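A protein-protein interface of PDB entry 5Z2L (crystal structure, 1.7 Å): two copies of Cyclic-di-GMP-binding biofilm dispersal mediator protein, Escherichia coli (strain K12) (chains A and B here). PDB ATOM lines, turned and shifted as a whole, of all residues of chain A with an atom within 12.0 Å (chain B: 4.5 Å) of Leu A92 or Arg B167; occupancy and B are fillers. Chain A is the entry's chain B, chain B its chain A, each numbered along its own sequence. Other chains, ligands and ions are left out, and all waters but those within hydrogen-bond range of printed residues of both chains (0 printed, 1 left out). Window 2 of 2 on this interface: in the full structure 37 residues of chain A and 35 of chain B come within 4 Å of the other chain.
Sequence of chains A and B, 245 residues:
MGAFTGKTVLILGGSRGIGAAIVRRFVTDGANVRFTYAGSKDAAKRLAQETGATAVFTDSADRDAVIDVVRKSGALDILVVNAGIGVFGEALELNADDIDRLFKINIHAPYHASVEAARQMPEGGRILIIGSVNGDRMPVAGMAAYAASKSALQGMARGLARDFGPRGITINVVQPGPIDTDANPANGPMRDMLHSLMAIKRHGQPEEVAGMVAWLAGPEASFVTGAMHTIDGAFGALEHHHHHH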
ATOM      1  N   VAL A  87     -10.135  18.919   0.638  1.00  0.00           N
ATOM      2  CA  VAL A  87      -9.193  17.814   0.705  1.00  0.00           C
ATOM      3  C   VAL A  87      -9.457  17.117   2.030  1.00  0.00           C
ATOM      4  O   VAL A  87      -9.198  17.688   3.095  1.00  0.00           O
ATOM      5  CB  VAL A  87      -7.743  18.293   0.601  1.00  0.00           C
ATOM      6  CG1 VAL A  87      -6.797  17.132   0.833  1.00  0.00           C
ATOM      7  CG2 VAL A  87      -7.507  18.922  -0.767  1.00  0.00           C
ATOM      8  N   PHE A  88     -10.002  15.904   1.973  1.00  0.00           N
ATOM      9  CA  PHE A  88     -10.519  15.249   3.167  1.00  0.00           C
ATOM     10  C   PHE A  88      -9.828  13.911   3.382  1.00  0.00           C
ATOM     11  O   PHE A  88      -9.517  13.191   2.425  1.00  0.00           O
ATOM     12  CB  PHE A  88     -12.041  15.057   3.079  1.00  0.00           C
ATOM     13  CG  PHE A  88     -12.791  16.332   2.830  1.00  0.00           C
ATOM     14  CD1 PHE A  88     -12.536  17.464   3.593  1.00  0.00           C
ATOM     15  CD2 PHE A  88     -13.766  16.404   1.846  1.00  0.00           C
ATOM     16  CE1 PHE A  88     -13.218  18.648   3.366  1.00  0.00           C
ATOM     17  CE2 PHE A  88     -14.464  17.592   1.623  1.00  0.00           C
ATOM     18  CZ  PHE A  88     -14.183  18.708   2.383  1.00  0.00           C
ATOM     19  N   GLY A  89      -9.613  13.581   4.643  1.00  0.00           N
ATOM     20  CA  GLY A  89      -8.965  12.340   5.020  1.00  0.00           C
ATOM     21  C   GLY A  89      -8.179  12.524   6.298  1.00  0.00           C
ATOM     22  O   GLY A  89      -8.040  13.623   6.823  1.00  0.00           O
ATOM     23  N   GLU A  90      -7.661  11.410   6.802  1.00  0.00           N
ATOM     24  CA  GLU A  90      -6.822  11.473   7.990  1.00  0.00           C
ATOM     25  C   GLU A  90      -5.644  12.407   7.734  1.00  0.00           C
ATOM     26  O   GLU A  90      -4.946  12.284   6.722  1.00  0.00           O
ATOM     27  CB  GLU A  90      -6.349  10.066   8.373  1.00  0.00           C
ATOM     28  CG  GLU A  90      -7.518   9.113   8.637  1.00  0.00           C
ATOM     29  CD  GLU A  90      -7.096   7.732   9.119  1.00  0.00           C
ATOM     30  OE1 GLU A  90      -5.876   7.467   9.227  1.00  0.00           O
ATOM     31  OE2 GLU A  90      -7.992   6.899   9.392  1.00  0.00           O
ATOM     32  N   ALA A  91      -5.443  13.365   8.645  1.00  0.00           N
ATOM     33  CA  ALA A  91      -4.413  14.380   8.444  1.00  0.00           C
ATOM     34  C   ALA A  91      -3.040  13.762   8.177  1.00  0.00           C
ATOM     35  O   ALA A  91      -2.273  14.280   7.358  1.00  0.00           O
ATOM     36  CB  ALA A  91      -4.352  15.312   9.654  1.00  0.00           C
ATOM     37  N   LEU A  92      -2.714  12.647   8.846  1.00  0.00           N
ATOM     38  CA  LEU A  92      -1.400  12.022   8.673  1.00  0.00           C
ATOM     39  C   LEU A  92      -1.247  11.287   7.346  1.00  0.00           C
ATOM     40  O   LEU A  92      -0.164  10.742   7.084  1.00  0.00           O
ATOM     41  CB  LEU A  92      -1.109  11.057   9.820  1.00  0.00           C
ATOM     42  CG  LEU A  92      -0.500  11.683  11.078  1.00  0.00           C
ATOM     43  CD1 LEU A  92      -1.414  12.728  11.665  1.00  0.00           C
ATOM     44  CD2 LEU A  92      -0.174  10.632  12.109  1.00  0.00           C
ATOM     45  N   GLU A  93      -2.282  11.249   6.504  1.00  0.00           N
ATOM     46  CA  GLU A  93      -2.198  10.574   5.217  1.00  0.00           C
ATOM     47  C   GLU A  93      -2.369  11.498   4.019  1.00  0.00           C
ATOM     48  O   GLU A  93      -2.158  11.051   2.886  1.00  0.00           O
ATOM     49  CB  GLU A  93      -3.244   9.454   5.132  1.00  0.00           C
ATOM     50  CG  GLU A  93      -3.127   8.416   6.240  1.00  0.00           C
ATOM     51  CD  GLU A  93      -4.005   7.201   5.994  1.00  0.00           C
ATOM     52  OE1 GLU A  93      -3.463   6.147   5.597  1.00  0.00           O
ATOM     53  OE2 GLU A  93      -5.237   7.305   6.189  1.00  0.00           O
ATOM     54  N   LEU A  94      -2.728  12.759   4.232  1.00  0.00           N
ATOM     55  CA  LEU A  94      -2.955  13.701   3.145  1.00  0.00           C
ATOM     56  C   LEU A  94      -1.634  14.274   2.638  1.00  0.00           C
ATOM     57  O   LEU A  94      -0.678  14.460   3.397  1.00  0.00           O
ATOM     58  CB  LEU A  94      -3.888  14.826   3.607  1.00  0.00           C
ATOM     59  CG  LEU A  94      -5.297  14.379   4.014  1.00  0.00           C
ATOM     60  CD1 LEU A  94      -6.132  15.560   4.574  1.00  0.00           C
ATOM     61  CD2 LEU A  94      -6.005  13.700   2.840  1.00  0.00           C
ATOM     62  N   ASN A  95      -1.582  14.532   1.332  1.00  0.00           N
ATOM     63  CA  ASN A  95      -0.382  15.069   0.703  1.00  0.00           C
ATOM     64  C   ASN A  95      -0.221  16.557   1.006  1.00  0.00           C
ATOM     65  O   ASN A  95      -1.173  17.332   0.872  1.00  0.00           O
ATOM     66  CB  ASN A  95      -0.438  14.844  -0.804  1.00  0.00           C
ATOM     67  CG  ASN A  95       0.736  15.456  -1.522  1.00  0.00           C
ATOM     68  OD1 ASN A  95       0.751  16.659  -1.798  1.00  0.00           O
ATOM     69  ND2 ASN A  95       1.741  14.648  -1.795  1.00  0.00           N
ATOM     70  N   ALA A  96       0.997  16.953   1.395  1.00  0.00           N
ATOM     71  CA  ALA A  96       1.245  18.328   1.831  1.00  0.00           C
ATOM     72  C   ALA A  96       1.003  19.334   0.712  1.00  0.00           C
ATOM     73  O   ALA A  96       0.510  20.445   0.967  1.00  0.00           O
ATOM     74  CB  ALA A  96       2.679  18.460   2.350  1.00  0.00           C
ATOM     75  N   ASP A  97       1.346  18.969  -0.531  1.00  0.00           N
ATOM     76  CA  ASP A  97       1.116  19.873  -1.655  1.00  0.00           C
ATOM     77  C   ASP A  97      -0.374  20.067  -1.903  1.00  0.00           C
ATOM     78  O   ASP A  97      -0.806  21.151  -2.320  1.00  0.00           O
ATOM     79  CB  ASP A  97       1.792  19.344  -2.923  1.00  0.00           C
ATOM     80  CG  ASP A  97       3.311  19.418  -2.861  1.00  0.00           C
ATOM     81  OD1 ASP A  97       3.982  18.533  -3.446  1.00  0.00           O
ATOM     82  OD2 ASP A  97       3.840  20.343  -2.218  1.00  0.00           O
ATOM     83  N   ASP A  98      -1.168  19.011  -1.697  1.00  0.00           N
ATOM     84  CA  ASP A  98      -2.617  19.144  -1.825  1.00  0.00           C
ATOM     85  C   ASP A  98      -3.166  20.083  -0.757  1.00  0.00           C
ATOM     86  O   ASP A  98      -4.018  20.942  -1.040  1.00  0.00           O
ATOM     87  CB  ASP A  98      -3.290  17.769  -1.727  1.00  0.00           C
ATOM     88  CG  ASP A  98      -2.939  16.855  -2.889  1.00  0.00           C
ATOM     89  OD1 ASP A  98      -2.534  17.370  -3.954  1.00  0.00           O
ATOM     90  OD2 ASP A  98      -3.072  15.618  -2.742  1.00  0.00           O
ATOM     91  N   ILE A  99      -2.674  19.944   0.479  1.00  0.00           N
ATOM     92  CA  ILE A  99      -3.108  20.836   1.554  1.00  0.00           C
ATOM     93  C   ILE A  99      -2.758  22.278   1.219  1.00  0.00           C
ATOM     94  O   ILE A  99      -3.584  23.183   1.365  1.00  0.00           O
ATOM     95  CB  ILE A  99      -2.492  20.418   2.900  1.00  0.00           C
ATOM     96  CG1 ILE A  99      -3.018  19.051   3.353  1.00  0.00           C
ATOM     97  CG2 ILE A  99      -2.779  21.497   3.956  1.00  0.00           C
ATOM     98  CD1 ILE A  99      -4.514  19.034   3.623  1.00  0.00           C
ATOM     99  N   VAL A 140     -15.678  17.234  11.724  1.00  0.00           N
ATOM    100  CA  VAL A 140     -15.485  15.789  11.778  1.00  0.00           C
ATOM    101  C   VAL A 140     -14.020  15.512  11.481  1.00  0.00           C
ATOM    102  O   VAL A 140     -13.291  16.393  11.008  1.00  0.00           O
ATOM    103  CB  VAL A 140     -16.394  15.048  10.785  1.00  0.00           C
ATOM    104  CG1 VAL A 140     -17.858  15.106  11.238  1.00  0.00           C
ATOM    105  CG2 VAL A 140     -16.238  15.663   9.413  1.00  0.00           C
ATOM    106  N   ALA A 141     -13.573  14.303  11.775  1.00  0.00           N
ATOM    107  CA  ALA A 141     -12.227  13.931  11.374  1.00  0.00           C
ATOM    108  C   ALA A 141     -12.078  14.091   9.866  1.00  0.00           C
ATOM    109  O   ALA A 141     -13.036  13.953   9.103  1.00  0.00           O
ATOM    110  CB  ALA A 141     -11.922  12.495  11.797  1.00  0.00           C
ATOM    111  N   GLY A 142     -10.867  14.417   9.438  1.00  0.00           N
ATOM    112  CA  GLY A 142     -10.560  14.411   8.030  1.00  0.00           C
ATOM    113  C   GLY A 142     -10.774  15.708   7.283  1.00  0.00           C
ATOM    114  O   GLY A 142     -10.633  15.714   6.056  1.00  0.00           O
ATOM    115  N   MET A 143     -11.086  16.810   7.967  1.00  0.00           N
ATOM    116  CA  MET A 143     -11.234  18.086   7.272  1.00  0.00           C
ATOM    117  C   MET A 143     -10.607  19.226   8.065  1.00  0.00           C
ATOM    118  O   MET A 143     -11.075  20.367   8.019  1.00  0.00           O
ATOM    119  CB  MET A 143     -12.699  18.384   6.983  1.00  0.00           C
ATOM    120  CG  MET A 143     -13.530  18.456   8.215  1.00  0.00           C
ATOM    121  SD  MET A 143     -14.983  19.448   7.874  1.00  0.00           S
ATOM    122  CE  MET A 143     -15.962  18.319   6.849  1.00  0.00           C
ATOM    123  N   ALA A 144      -9.498  18.948   8.754  1.00  0.00           N
ATOM    124  CA  ALA A 144      -8.890  19.961   9.611  1.00  0.00           C
ATOM    125  C   ALA A 144      -8.393  21.155   8.795  1.00  0.00           C
ATOM    126  O   ALA A 144      -8.661  22.313   9.144  1.00  0.00           O
ATOM    127  CB  ALA A 144      -7.757  19.332  10.424  1.00  0.00           C
ATOM    128  N   ALA A 145      -7.663  20.898   7.703  1.00  0.00           N
ATOM    129  CA  ALA A 145      -7.176  22.001   6.877  1.00  0.00           C
ATOM    130  C   ALA A 145      -8.328  22.765   6.224  1.00  0.00           C
ATOM    131  O   ALA A 145      -8.308  23.997   6.167  1.00  0.00           O
ATOM    132  CB  ALA A 145      -6.205  21.480   5.816  1.00  0.00           C
ATOM    133  N   TYR A 146      -9.350  22.055   5.738  1.00  0.00           N
ATOM    134  CA  TYR A 146     -10.514  22.730   5.170  1.00  0.00           C
ATOM    135  C   TYR A 146     -11.169  23.646   6.201  1.00  0.00           C
ATOM    136  O   TYR A 146     -11.482  24.818   5.919  1.00  0.00           O
ATOM    137  CB  TYR A 146     -11.512  21.689   4.656  1.00  0.00           C
ATOM    138  CG  TYR A 146     -12.820  22.278   4.154  1.00  0.00           C
ATOM    139  CD1 TYR A 146     -12.898  22.857   2.892  1.00  0.00           C
ATOM    140  CD2 TYR A 146     -13.979  22.245   4.931  1.00  0.00           C
ATOM    141  CE1 TYR A 146     -14.084  23.387   2.414  1.00  0.00           C
ATOM    142  CE2 TYR A 146     -15.177  22.772   4.457  1.00  0.00           C
ATOM    143  CZ  TYR A 146     -15.216  23.341   3.196  1.00  0.00           C
ATOM    144  OH  TYR A 146     -16.383  23.886   2.690  1.00  0.00           O
ATOM    145  N   VAL B 115       0.895  18.205  12.345  1.00  0.00           N
ATOM    146  CA  VAL B 115       0.697  16.867  11.779  1.00  0.00           C
ATOM    147  C   VAL B 115       1.986  16.045  11.879  1.00  0.00           C
ATOM    148  O   VAL B 115       1.990  14.877  12.333  1.00  0.00           O
ATOM    149  CB  VAL B 115       0.207  16.980  10.323  1.00  0.00           C
ATOM    150  CG1 VAL B 115       0.180  15.607   9.632  1.00  0.00           C
ATOM    151  CG2 VAL B 115      -1.153  17.696  10.260  1.00  0.00           C
ATOM    152  N   ALA B 118       2.684  14.800  15.269  1.00  0.00           N
ATOM    153  CA  ALA B 118       1.811  13.692  15.627  1.00  0.00           C
ATOM    154  C   ALA B 118       2.299  12.368  15.048  1.00  0.00           C
ATOM    155  O   ALA B 118       1.908  11.310  15.552  1.00  0.00           O
ATOM    156  CB  ALA B 118       0.373  13.969  15.165  1.00  0.00           C
ATOM    157  N   ARG B 119       3.159  12.385  14.022  1.00  0.00           N
ATOM    158  CA  ARG B 119       3.630  11.094  13.497  1.00  0.00           C
ATOM    159  C   ARG B 119       4.369  10.258  14.551  1.00  0.00           C
ATOM    160  O   ARG B 119       4.253   9.026  14.558  1.00  0.00           O
ATOM    161  CB  ARG B 119       4.527  11.284  12.273  1.00  0.00           C
ATOM    162  CG  ARG B 119       3.800  11.910  11.098  1.00  0.00           C
ATOM    163  CD  ARG B 119       4.595  11.790   9.804  1.00  0.00           C
ATOM    164  NE  ARG B 119       4.059  12.720   8.821  1.00  0.00           N
ATOM    165  CZ  ARG B 119       2.942  12.510   8.134  1.00  0.00           C
ATOM    166  NH1 ARG B 119       2.259  11.387   8.307  1.00  0.00           N
ATOM    167  NH2 ARG B 119       2.513  13.420   7.272  1.00  0.00           N
ATOM    168  N   MET B 121       4.626  11.304  18.089  1.00  0.00           N
ATOM    169  CA  MET B 121       4.313  11.700  19.449  1.00  0.00           C
ATOM    170  C   MET B 121       3.543  10.591  20.163  1.00  0.00           C
ATOM    171  O   MET B 121       2.610  10.017  19.584  1.00  0.00           O
ATOM    172  CB  MET B 121       3.507  12.995  19.401  1.00  0.00           C
ATOM    173  CG  MET B 121       3.146  13.568  20.733  1.00  0.00           C
ATOM    174  SD  MET B 121       2.391  15.190  20.484  1.00  0.00           S
ATOM    175  CE  MET B 121       3.854  16.209  20.392  1.00  0.00           C
ATOM    176  N   PRO B 122       3.896  10.259  21.401  1.00  0.00           N
ATOM    177  CA  PRO B 122       3.224   9.170  22.118  1.00  0.00           C
ATOM    178  C   PRO B 122       1.881   9.606  22.691  1.00  0.00           C
ATOM    179  O   PRO B 122       1.504  10.778  22.659  1.00  0.00           O
ATOM    180  CB  PRO B 122       4.188   8.873  23.260  1.00  0.00           C
ATOM    181  CG  PRO B 122       4.764  10.225  23.569  1.00  0.00           C
ATOM    182  CD  PRO B 122       4.954  10.878  22.218  1.00  0.00           C
ATOM    183  N   GLU B 123       1.172   8.624  23.252  1.00  0.00           N
ATOM    184  CA  GLU B 123      -0.023   8.926  24.030  1.00  0.00           C
ATOM    185  C   GLU B 123       0.349   9.823  25.199  1.00  0.00           C
ATOM    186  O   GLU B 123       1.346   9.591  25.886  1.00  0.00           O
ATOM    187  CB  GLU B 123      -0.673   7.644  24.552  1.00  0.00           C
ATOM    188  CG  GLU B 123      -1.299   6.767  23.473  1.00  0.00           C
ATOM    189  CD  GLU B 123      -2.031   5.568  24.052  1.00  0.00           C
ATOM    190  OE1 GLU B 123      -1.785   5.225  25.229  1.00  0.00           O
ATOM    191  OE2 GLU B 123      -2.855   4.968  23.331  1.00  0.00           O
ATOM    192  N   PHE B 164      -6.295  13.750  16.055  1.00  0.00           N
ATOM    193  CA  PHE B 164      -5.279  13.309  17.006  1.00  0.00           C
ATOM    194  C   PHE B 164      -5.852  12.609  18.229  1.00  0.00           C
ATOM    195  O   PHE B 164      -5.097  11.955  18.957  1.00  0.00           O
ATOM    196  CB  PHE B 164      -4.447  14.500  17.501  1.00  0.00           C
ATOM    197  CG  PHE B 164      -3.662  15.202  16.420  1.00  0.00           C
ATOM    198  CD1 PHE B 164      -3.431  14.590  15.198  1.00  0.00           C
ATOM    199  CD2 PHE B 164      -3.178  16.489  16.629  1.00  0.00           C
ATOM    200  CE1 PHE B 164      -2.714  15.246  14.205  1.00  0.00           C
ATOM    201  CE2 PHE B 164      -2.471  17.153  15.645  1.00  0.00           C
ATOM    202  CZ  PHE B 164      -2.226  16.518  14.428  1.00  0.00           C
ATOM    203  N   GLY B 165      -7.155  12.734  18.476  1.00  0.00           N
ATOM    204  CA  GLY B 165      -7.768  12.128  19.637  1.00  0.00           C
ATOM    205  C   GLY B 165      -7.446  10.658  19.828  1.00  0.00           C
ATOM    206  O   GLY B 165      -7.065  10.231  20.920  1.00  0.00           O
ATOM    207  N   PRO B 166      -7.610   9.848  18.776  1.00  0.00           N
ATOM    208  CA  PRO B 166      -7.290   8.417  18.898  1.00  0.00           C
ATOM    209  C   PRO B 166      -5.849   8.145  19.269  1.00  0.00           C
ATOM    210  O   PRO B 166      -5.548   7.055  19.773  1.00  0.00           O
ATOM    211  CB  PRO B 166      -7.616   7.860  17.504  1.00  0.00           C
ATOM    212  CG  PRO B 166      -8.565   8.817  16.919  1.00  0.00           C
ATOM    213  CD  PRO B 166      -8.172  10.170  17.451  1.00  0.00           C
ATOM    214  N   ARG B 167      -4.946   9.089  19.030  1.00  0.00           N
ATOM    215  CA  ARG B 167      -3.541   8.888  19.357  1.00  0.00           C
ATOM    216  C   ARG B 167      -3.207   9.347  20.769  1.00  0.00           C
ATOM    217  O   ARG B 167      -2.049   9.230  21.188  1.00  0.00           O
ATOM    218  CB  ARG B 167      -2.654   9.628  18.349  1.00  0.00           C
ATOM    219  CG  ARG B 167      -3.006   9.347  16.894  1.00  0.00           C
ATOM    220  CD  ARG B 167      -1.966   9.938  15.948  1.00  0.00           C
ATOM    221  NE  ARG B 167      -1.484   8.958  14.975  1.00  0.00           N
ATOM    222  CZ  ARG B 167      -0.413   8.191  15.143  1.00  0.00           C
ATOM    223  NH1 ARG B 167       0.309   8.275  16.253  1.00  0.00           N
ATOM    224  NH2 ARG B 167      -0.061   7.333  14.195  1.00  0.00           N
ATOM    225  N   GLY B 168      -4.192   9.853  21.513  1.00  0.00           N
ATOM    226  CA  GLY B 168      -3.932  10.324  22.855  1.00  0.00           C
ATOM    227  C   GLY B 168      -3.224  11.652  22.925  1.00  0.00           C
ATOM    228  O   GLY B 168      -2.596  11.951  23.939  1.00  0.00           O
ATOM    229  N   ILE B 169      -3.326  12.466  21.879  1.00  0.00           N
ATOM    230  CA  ILE B 169      -2.655  13.754  21.794  1.00  0.00           C
ATOM    231  C   ILE B 169      -3.712  14.850  21.863  1.00  0.00           C
ATOM    232  O   ILE B 169      -4.731  14.764  21.168  1.00  0.00           O
ATOM    233  CB  ILE B 169      -1.863  13.868  20.484  1.00  0.00           C
ATOM    234  CG1 ILE B 169      -0.769  12.796  20.403  1.00  0.00           C
ATOM    235  CG2 ILE B 169      -1.308  15.278  20.329  1.00  0.00           C
ATOM    236  CD1 ILE B 169      -0.164  12.654  19.005  1.00  0.00           C
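The guanidinium group of Arg B119 is in hydrogen-bond range of the backbone carbonyl oxygen of Leu A92 (2.8 Å).
The backbone carbonyl oxygen (O) of Phe B164 lies within hydrogen-bond range of the backbone NH (N) of Ile B169.
Ala A91 touches Val B115 (O to CG1, 3.6 Å). Val B115 touches Leu A92. CD1 of Leu A92 touches CE1 of Phe B164 (3.8 Å). Arg B167 touches Leu A92.
Of chain A, only Leu A92 comes within 4 Å of Arg B167. Val B115 touches two residues of chain A. Of the printed residues of chain A, Arg B119 touches Leu A92 (2.8 Å). No residue of chain A comes within 4 Å of Pro B122. Phe B164 touches just one residue of chain A: Leu A92 (3.8 Å). Gly B165 touches none of the printed residues of chain A. No residue of chain A comes within 4 Å of Pro B166. No residue of chain A comes within 4 Å of Gly B168. No residue of chain A comes within 4 Å of Ile B169. Printed residues of chain B within 4 Å of Ala A91: Val B115. Asp A98 touches none of the printed residues of chain B.
Hydrophobic or aromatic side chains of chain B within 4 Å of the printed part of chain A: Val B115 and Phe B164. Printed residues of chain A that touch a printed residue of chain B: Ala A91 and Leu A92. Among the printed residues, no Asp or Glu carboxylate lies within 4 Å of a Lys or Arg side-chain nitrogen of the other chain.
No position is printed for both chains. Of the 5 pairs that touch across the chains among the printed residues, none has its exchanged pair printed and touching as well.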
